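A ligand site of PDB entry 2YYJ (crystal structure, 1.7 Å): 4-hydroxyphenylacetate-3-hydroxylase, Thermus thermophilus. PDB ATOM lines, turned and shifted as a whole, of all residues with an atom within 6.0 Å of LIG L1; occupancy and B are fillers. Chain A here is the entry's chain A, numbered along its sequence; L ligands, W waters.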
ATOM      1  N   ARG A 100       6.618 -18.887 -12.849  1.00  0.00           N
ATOM      2  CA  ARG A 100       7.130 -20.245 -12.757  1.00  0.00           C
ATOM      3  C   ARG A 100       6.613 -21.230 -13.797  1.00  0.00           C
ATOM      4  O   ARG A 100       6.250 -22.364 -13.461  1.00  0.00           O
ATOM      5  CB  ARG A 100       6.874 -20.807 -11.352  1.00  0.00           C
ATOM      6  CG  ARG A 100       8.064 -20.665 -10.411  1.00  0.00           C
ATOM      7  CD  ARG A 100       8.357 -19.224 -10.044  1.00  0.00           C
ATOM      8  NE  ARG A 100       9.689 -19.077  -9.446  1.00  0.00           N
ATOM      9  CZ  ARG A 100      10.825 -19.086 -10.144  1.00  0.00           C
ATOM     10  NH1 ARG A 100      10.795 -19.221 -11.458  1.00  0.00           N
ATOM     11  NH2 ARG A 100      11.989 -18.971  -9.523  1.00  0.00           N
ATOM     12  N   TYR A 104      11.344 -22.981 -17.047  1.00  0.00           N
ATOM     13  CA  TYR A 104      12.404 -22.472 -16.176  1.00  0.00           C
ATOM     14  C   TYR A 104      13.087 -23.672 -15.519  1.00  0.00           C
ATOM     15  O   TYR A 104      14.312 -23.768 -15.492  1.00  0.00           O
ATOM     16  CB  TYR A 104      11.793 -21.558 -15.115  1.00  0.00           C
ATOM     17  CG  TYR A 104      12.714 -21.142 -13.979  1.00  0.00           C
ATOM     18  CD1 TYR A 104      13.652 -20.112 -14.131  1.00  0.00           C
ATOM     19  CD2 TYR A 104      12.596 -21.731 -12.720  1.00  0.00           C
ATOM     20  CE1 TYR A 104      14.426 -19.677 -13.062  1.00  0.00           C
ATOM     21  CE2 TYR A 104      13.375 -21.303 -11.646  1.00  0.00           C
ATOM     22  CZ  TYR A 104      14.285 -20.269 -11.823  1.00  0.00           C
ATOM     23  OH  TYR A 104      15.009 -19.809 -10.740  1.00  0.00           O
ATOM     24  N   LEU A 105      12.281 -24.592 -14.988  1.00  0.00           N
ATOM     25  CA  LEU A 105      12.818 -25.767 -14.327  1.00  0.00           C
ATOM     26  C   LEU A 105      13.339 -26.797 -15.330  1.00  0.00           C
ATOM     27  O   LEU A 105      14.244 -27.573 -15.007  1.00  0.00           O
ATOM     28  CB  LEU A 105      11.757 -26.399 -13.416  1.00  0.00           C
ATOM     29  CG  LEU A 105      11.357 -25.523 -12.225  1.00  0.00           C
ATOM     30  CD1 LEU A 105      10.289 -26.224 -11.383  1.00  0.00           C
ATOM     31  CD2 LEU A 105      12.589 -25.232 -11.369  1.00  0.00           C
ATOM     32  N   HIS A 142       8.863 -26.361  -7.816  1.00  0.00           N
ATOM     33  CA  HIS A 142      10.065 -26.569  -7.010  1.00  0.00           C
ATOM     34  C   HIS A 142      10.088 -25.753  -5.735  1.00  0.00           C
ATOM     35  O   HIS A 142       9.368 -24.758  -5.619  1.00  0.00           O
ATOM     36  CB  HIS A 142      11.318 -26.250  -7.839  1.00  0.00           C
ATOM     37  CG  HIS A 142      11.561 -24.784  -8.028  1.00  0.00           C
ATOM     38  ND1 HIS A 142      10.582 -23.922  -8.501  1.00  0.00           N
ATOM     39  CD2 HIS A 142      12.659 -24.027  -7.820  1.00  0.00           C
ATOM     40  CE1 HIS A 142      11.085 -22.705  -8.575  1.00  0.00           C
ATOM     41  NE2 HIS A 142      12.341 -22.737  -8.161  1.00  0.00           N
ATOM     42  N   LEU A 144      13.230 -24.597  -2.883  1.00  0.00           N
ATOM     43  CA  LEU A 144      14.642 -24.654  -2.496  1.00  0.00           C
ATOM     44  C   LEU A 144      14.984 -24.071  -1.132  1.00  0.00           C
ATOM     45  O   LEU A 144      16.116 -24.221  -0.671  1.00  0.00           O
ATOM     46  CB  LEU A 144      15.489 -23.902  -3.530  1.00  0.00           C
ATOM     47  CG  LEU A 144      15.219 -24.127  -5.023  1.00  0.00           C
ATOM     48  CD1 LEU A 144      16.250 -23.344  -5.833  1.00  0.00           C
ATOM     49  CD2 LEU A 144      15.303 -25.597  -5.356  1.00  0.00           C
ATOM     50  N   THR A 145      14.028 -23.401  -0.501  1.00  0.00           N
ATOM     51  CA  THR A 145      14.314 -22.756   0.774  1.00  0.00           C
ATOM     52  C   THR A 145      13.739 -23.411   2.021  1.00  0.00           C
ATOM     53  O   THR A 145      12.694 -24.067   1.979  1.00  0.00           O
ATOM     54  CB  THR A 145      13.859 -21.277   0.734  1.00  0.00           C
ATOM     55  OG1 THR A 145      12.427 -21.207   0.736  1.00  0.00           O
ATOM     56  CG2 THR A 145      14.375 -20.606  -0.533  1.00  0.00           C
ATOM     57  N   PRO A 196      18.847 -28.120  -4.059  1.00  0.00           N
ATOM     58  CA  PRO A 196      19.598 -27.237  -3.167  1.00  0.00           C
ATOM     59  C   PRO A 196      19.342 -25.765  -3.508  1.00  0.00           C
ATOM     60  O   PRO A 196      18.749 -25.454  -4.537  1.00  0.00           O
ATOM     61  CB  PRO A 196      21.062 -27.607  -3.445  1.00  0.00           C
ATOM     62  CG  PRO A 196      20.976 -28.986  -4.030  1.00  0.00           C
ATOM     63  CD  PRO A 196      19.753 -28.918  -4.887  1.00  0.00           C
ATOM     64  N   SER A 197      19.807 -24.881  -2.633  1.00  0.00           N
ATOM     65  CA  SER A 197      19.657 -23.452  -2.868  1.00  0.00           C
ATOM     66  C   SER A 197      20.644 -23.040  -3.973  1.00  0.00           C
ATOM     67  O   SER A 197      21.651 -23.714  -4.189  1.00  0.00           O
ATOM     68  CB  SER A 197      19.969 -22.681  -1.593  1.00  0.00           C
ATOM     69  OG  SER A 197      20.165 -21.298  -1.869  1.00  0.00           O
ATOM     70  N   THR A 198      20.344 -21.942  -4.645  1.00  0.00           N
ATOM     71  CA  THR A 198      21.217 -21.440  -5.702  1.00  0.00           C
ATOM     72  C   THR A 198      22.288 -20.511  -5.127  1.00  0.00           C
ATOM     73  O   THR A 198      23.175 -20.074  -5.856  1.00  0.00           O
ATOM     74  CB  THR A 198      20.445 -20.646  -6.774  1.00  0.00           C
ATOM     75  OG1 THR A 198      19.872 -19.479  -6.175  1.00  0.00           O
ATOM     76  CG2 THR A 198      19.337 -21.500  -7.388  1.00  0.00           C
ATOM     77  N   LEU A 199      22.209 -20.206  -3.831  1.00  0.00           N
ATOM     78  CA  LEU A 199      23.207 -19.327  -3.224  1.00  0.00           C
ATOM     79  C   LEU A 199      23.525 -19.574  -1.759  1.00  0.00           C
ATOM     80  O   LEU A 199      24.598 -19.182  -1.284  1.00  0.00           O
ATOM     81  CB  LEU A 199      22.811 -17.843  -3.398  1.00  0.00           C
ATOM     82  CG  LEU A 199      21.731 -17.267  -2.483  1.00  0.00           C
ATOM     83  CD1 LEU A 199      21.763 -15.735  -2.529  1.00  0.00           C
ATOM     84  CD2 LEU A 199      20.373 -17.767  -2.913  1.00  0.00           C
ATOM     85  N   LEU A 200      22.621 -20.208  -1.015  1.00  0.00           N
ATOM     86  CA  LEU A 200      22.857 -20.481   0.400  1.00  0.00           C
ATOM     87  C   LEU A 200      23.538 -21.829   0.624  1.00  0.00           C
ATOM     88  O   LEU A 200      23.300 -22.777  -0.109  1.00  0.00           O
ATOM     89  CB  LEU A 200      21.542 -20.444   1.177  1.00  0.00           C
ATOM     90  CG  LEU A 200      20.700 -19.169   1.044  1.00  0.00           C
ATOM     91  CD1 LEU A 200      19.469 -19.273   1.936  1.00  0.00           C
ATOM     92  CD2 LEU A 200      21.519 -17.938   1.420  1.00  0.00           C
ATOM     93  N   MET A 284      18.822 -21.364 -16.291  1.00  0.00           N
ATOM     94  CA  MET A 284      17.594 -20.936 -15.635  1.00  0.00           C
ATOM     95  C   MET A 284      17.530 -19.400 -15.656  1.00  0.00           C
ATOM     96  O   MET A 284      16.458 -18.828 -15.813  1.00  0.00           O
ATOM     97  CB  MET A 284      17.519 -21.482 -14.199  1.00  0.00           C
ATOM     98  CG  MET A 284      18.487 -20.856 -13.202  1.00  0.00           C
ATOM     99  SD  MET A 284      18.844 -21.975 -11.810  1.00  0.00           S
ATOM    100  CE  MET A 284      17.301 -21.941 -10.900  1.00  0.00           C
ATOM    101  N   PHE A 440      12.378 -10.894  -4.647  1.00  0.00           N
ATOM    102  CA  PHE A 440      12.951 -12.069  -3.997  1.00  0.00           C
ATOM    103  C   PHE A 440      13.037 -13.446  -4.672  1.00  0.00           C
ATOM    104  O   PHE A 440      13.774 -14.300  -4.194  1.00  0.00           O
ATOM    105  CB  PHE A 440      12.209 -12.303  -2.670  1.00  0.00           C
ATOM    106  CG  PHE A 440      12.562 -11.334  -1.591  1.00  0.00           C
ATOM    107  CD1 PHE A 440      13.813 -11.380  -0.992  1.00  0.00           C
ATOM    108  CD2 PHE A 440      11.634 -10.392  -1.149  1.00  0.00           C
ATOM    109  CE1 PHE A 440      14.144 -10.512   0.046  1.00  0.00           C
ATOM    110  CE2 PHE A 440      11.949  -9.517  -0.108  1.00  0.00           C
ATOM    111  CZ  PHE A 440      13.208  -9.574   0.489  1.00  0.00           C
ATOM    112  N   PHE A 441      12.297 -13.674  -5.742  1.00  0.00           N
ATOM    113  CA  PHE A 441      12.298 -15.019  -6.305  1.00  0.00           C
ATOM    114  C   PHE A 441      13.653 -15.714  -6.504  1.00  0.00           C
ATOM    115  O   PHE A 441      13.782 -16.897  -6.205  1.00  0.00           O
ATOM    116  CB  PHE A 441      11.468 -15.069  -7.594  1.00  0.00           C
ATOM    117  CG  PHE A 441      12.241 -14.762  -8.834  1.00  0.00           C
ATOM    118  CD1 PHE A 441      13.005 -15.746  -9.460  1.00  0.00           C
ATOM    119  CD2 PHE A 441      12.228 -13.487  -9.381  1.00  0.00           C
ATOM    120  CE1 PHE A 441      13.748 -15.457 -10.598  1.00  0.00           C
ATOM    121  CE2 PHE A 441      12.963 -13.186 -10.517  1.00  0.00           C
ATOM    122  CZ  PHE A 441      13.720 -14.176 -11.129  1.00  0.00           C
ATOM    123  N   PHE A 442      14.668 -14.984  -6.967  1.00  0.00           N
ATOM    124  CA  PHE A 442      15.993 -15.582  -7.205  1.00  0.00           C
ATOM    125  C   PHE A 442      16.884 -15.556  -5.953  1.00  0.00           C
ATOM    126  O   PHE A 442      18.030 -16.036  -5.983  1.00  0.00           O
ATOM    127  CB  PHE A 442      16.702 -14.867  -8.355  1.00  0.00           C
ATOM    128  CG  PHE A 442      17.267 -15.803  -9.405  1.00  0.00           C
ATOM    129  CD1 PHE A 442      17.306 -15.413 -10.735  1.00  0.00           C
ATOM    130  CD2 PHE A 442      17.773 -17.051  -9.061  1.00  0.00           C
ATOM    131  CE1 PHE A 442      17.826 -16.253 -11.716  1.00  0.00           C
ATOM    132  CE2 PHE A 442      18.302 -17.904 -10.029  1.00  0.00           C
ATOM    133  CZ  PHE A 442      18.333 -17.502 -11.357  1.00  0.00           C
ATOM    134  N   GLY A 443      16.352 -15.024  -4.867  1.00  0.00           N
ATOM    135  CA  GLY A 443      17.112 -14.961  -3.626  1.00  0.00           C
ATOM    136  C   GLY A 443      17.088 -13.591  -2.987  1.00  0.00           C
ATOM    137  O   GLY A 443      16.613 -12.622  -3.586  1.00  0.00           O
HETATM  138  C1  LIG L   1      17.546 -19.877  -3.171  1.00  0.00           C
HETATM  139  O1  LIG L   1      18.252 -20.329  -4.056  1.00  0.00           O
HETATM  140  O2  LIG L   1      17.931 -20.008  -1.911  1.00  0.00           O
HETATM  141  C2  LIG L   1      16.227 -19.176  -3.482  1.00  0.00           C
HETATM  142  C3  LIG L   1      15.730 -19.517  -4.867  1.00  0.00           C
HETATM  143  C4  LIG L   1      16.374 -19.097  -6.054  1.00  0.00           C
HETATM  144  C5  LIG L   1      15.845 -19.486  -7.303  1.00  0.00           C
HETATM  145  C6  LIG L   1      14.671 -20.296  -7.365  1.00  0.00           C
HETATM  146  C7  LIG L   1      14.040 -20.700  -6.170  1.00  0.00           C
HETATM  147  C8  LIG L   1      14.568 -20.310  -4.935  1.00  0.00           C
HETATM  148  O3  LIG L   1      14.158 -20.685  -8.544  1.00  0.00           O
HETATM  149  P1  LG2 L   2      14.959 -14.627   4.748  1.00  0.00           P
HETATM  150  O1  LG2 L   2      16.257 -15.348   4.710  1.00  0.00           O
HETATM  151  O2  LG2 L   2      13.982 -15.181   5.712  1.00  0.00           O
HETATM  152  O3  LG2 L   2      15.134 -13.086   5.178  1.00  0.00           O
HETATM  153  C1  LG2 L   2      14.219 -12.181   5.816  1.00  0.00           C
HETATM  154  C2  LG2 L   2      15.037 -10.894   5.976  1.00  0.00           C
HETATM  155  O4  LG2 L   2      16.091 -11.331   6.844  1.00  0.00           O
HETATM  156  C3  LG2 L   2      15.671 -10.138   4.808  1.00  0.00           C
HETATM  157  O5  LG2 L   2      15.737  -8.737   5.104  1.00  0.00           O
HETATM  158  C4  LG2 L   2      17.058 -10.780   4.724  1.00  0.00           C
HETATM  159  O6  LG2 L   2      18.004  -9.923   4.073  1.00  0.00           O
HETATM  160  C5  LG2 L   2      17.345 -11.071   6.196  1.00  0.00           C
HETATM  161  N1  LG2 L   2      18.400 -12.037   6.616  1.00  0.00           N
HETATM  162  C6  LG2 L   2      18.148 -13.313   6.901  1.00  0.00           C
HETATM  163  N2  LG2 L   2      19.264 -14.029   6.855  1.00  0.00           N
HETATM  164  C7  LG2 L   2      20.259 -13.195   6.567  1.00  0.00           C
HETATM  165  C8  LG2 L   2      21.635 -13.340   6.431  1.00  0.00           C
HETATM  166  N3  LG2 L   2      22.225 -14.508   6.651  1.00  0.00           N
HETATM  167  N4  LG2 L   2      22.373 -12.252   6.127  1.00  0.00           N
HETATM  168  C9  LG2 L   2      21.832 -11.061   5.961  1.00  0.00           C
HETATM  169  N5  LG2 L   2      20.524 -10.893   6.106  1.00  0.00           N
HETATM  170  C10 LG2 L   2      19.716 -11.925   6.421  1.00  0.00           C
HETATM  171  N6  LG2 L   2      11.343 -20.286  -3.517  1.00  0.00           N
HETATM  172  C11 LG2 L   2      11.376 -21.554  -4.120  1.00  0.00           C
HETATM  173  O7  LG2 L   2      12.184 -22.399  -3.749  1.00  0.00           O
HETATM  174  N7  LG2 L   2      10.458 -21.833  -5.146  1.00  0.00           N
HETATM  175  C12 LG2 L   2       9.512 -20.869  -5.550  1.00  0.00           C
HETATM  176  O8  LG2 L   2       8.743 -21.129  -6.469  1.00  0.00           O
HETATM  177  C13 LG2 L   2       9.445 -19.636  -4.910  1.00  0.00           C
HETATM  178  N8  LG2 L   2       8.483 -18.655  -5.203  1.00  0.00           N
HETATM  179  C14 LG2 L   2       8.380 -17.421  -4.552  1.00  0.00           C
HETATM  180  C15 LG2 L   2       7.330 -16.544  -4.858  1.00  0.00           C
HETATM  181  C16 LG2 L   2       7.190 -15.358  -4.149  1.00  0.00           C
HETATM  182  C17 LG2 L   2       5.970 -14.498  -4.495  1.00  0.00           C
HETATM  183  C18 LG2 L   2       8.116 -15.002  -3.161  1.00  0.00           C
HETATM  184  C19 LG2 L   2       8.178 -13.714  -2.345  1.00  0.00           C
HETATM  185  C20 LG2 L   2       9.142 -15.899  -2.875  1.00  0.00           C
HETATM  186  C21 LG2 L   2       9.294 -17.135  -3.532  1.00  0.00           C
HETATM  187  N9  LG2 L   2      10.265 -18.112  -3.225  1.00  0.00           N
HETATM  188  C22 LG2 L   2      10.366 -19.345  -3.890  1.00  0.00           C
HETATM  189  C23 LG2 L   2      11.279 -17.852  -2.176  1.00  0.00           C
HETATM  190  C24 LG2 L   2      12.454 -16.908  -2.447  1.00  0.00           C
HETATM  191  O9  LG2 L   2      13.479 -17.567  -3.198  1.00  0.00           O
HETATM  192  C25 LG2 L   2      12.890 -16.341  -1.087  1.00  0.00           C
HETATM  193  O10 LG2 L   2      11.940 -15.381  -0.627  1.00  0.00           O
HETATM  194  C26 LG2 L   2      14.251 -15.633  -1.141  1.00  0.00           C
HETATM  195  O11 LG2 L   2      15.240 -16.561  -1.595  1.00  0.00           O
HETATM  196  C27 LG2 L   2      14.855 -14.987   0.113  1.00  0.00           C
HETATM  197  O12 LG2 L   2      14.871 -15.853   1.256  1.00  0.00           O
HETATM  198  P2  LG2 L   2      13.721 -15.800   2.388  1.00  0.00           P
HETATM  199  O13 LG2 L   2      12.379 -15.416   1.904  1.00  0.00           O
HETATM  200  O14 LG2 L   2      13.866 -17.100   3.090  1.00  0.00           O
HETATM  201  O15 LG2 L   2      13.999 -14.623   3.449  1.00  0.00           O
HETATM  202  O   HOH W   1      11.781 -18.576  -6.892  1.00  0.00           O
HETATM  203  O   HOH W   2      17.028 -18.174  -0.181  1.00  0.00           O
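Water W2 lies within hydrogen-bond range of an oxygen (O2) of LIG L1 (2.7 Å) and an oxygen (O11) of LG2 L2 (2.8 Å). Water W1 lies within hydrogen-bond range of the guanidinium group of Arg 100 (2.7 Å) and the backbone carbonyl oxygen of Phe 441 (2.7 Å).
OH of Tyr 104 lies within hydrogen-bond range of NH2 of Arg 100 (3.4 Å). The side-chain hydroxyl (OG) of Ser 197 is in hydrogen-bond range of the backbone NH (N) of Leu 199 (3.0 Å). OG of Ser 197 lies within hydrogen-bond range of N of Leu 200 (2.8 Å).
A ring nitrogen (NE2) of His 142 is in hydrogen-bond range of an oxygen (O3) of LIG L1 (2.8 Å). The backbone NH of Leu 144 lies within hydrogen-bond range of an oxygen (O7) of LG2 L2 (2.6 Å). An oxygen (O1) of LIG L1 is in hydrogen-bond range of the backbone NH of Thr 198, 2.7 Å away. The side-chain hydroxyl (OG1) of Thr 198 lies within hydrogen-bond range of an oxygen (O1) of LIG L1 (2.8 Å). The backbone carbonyl oxygen (O) of Phe 441 is in hydrogen-bond range of an oxygen (O9) of LG2 L2 (3.1 Å). O of Phe 440 sits close to O9 of LG2 L2 (3.4 Å). The side-chain hydroxyl of Tyr 104 sits at hydrogen-bond distance from an oxygen (O3) of LIG L1 (2.5 Å). O of His 142 lies within hydrogen-bond range of N7 of LG2 L2. The side-chain hydroxyl (OG) of Ser 197 sits at hydrogen-bond distance from an oxygen (O2) of LIG L1 (2.6 Å). An oxygen (O3) of LIG L1 sits at hydrogen-bond distance from the guanidinium group of Arg 100 (2.9 Å).
Residues that only touch LIG L1: Leu 144 (3.5 Å), Thr 145 (3.8 Å), Leu 199 (3.5 Å), Phe 441 (3.4 Å) and Phe 442 (3.5 Å). Hydrophobic or aromatic side chains that line LIG L1: Tyr 104, His 142, Leu 144, Leu 199 and Phe 442.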
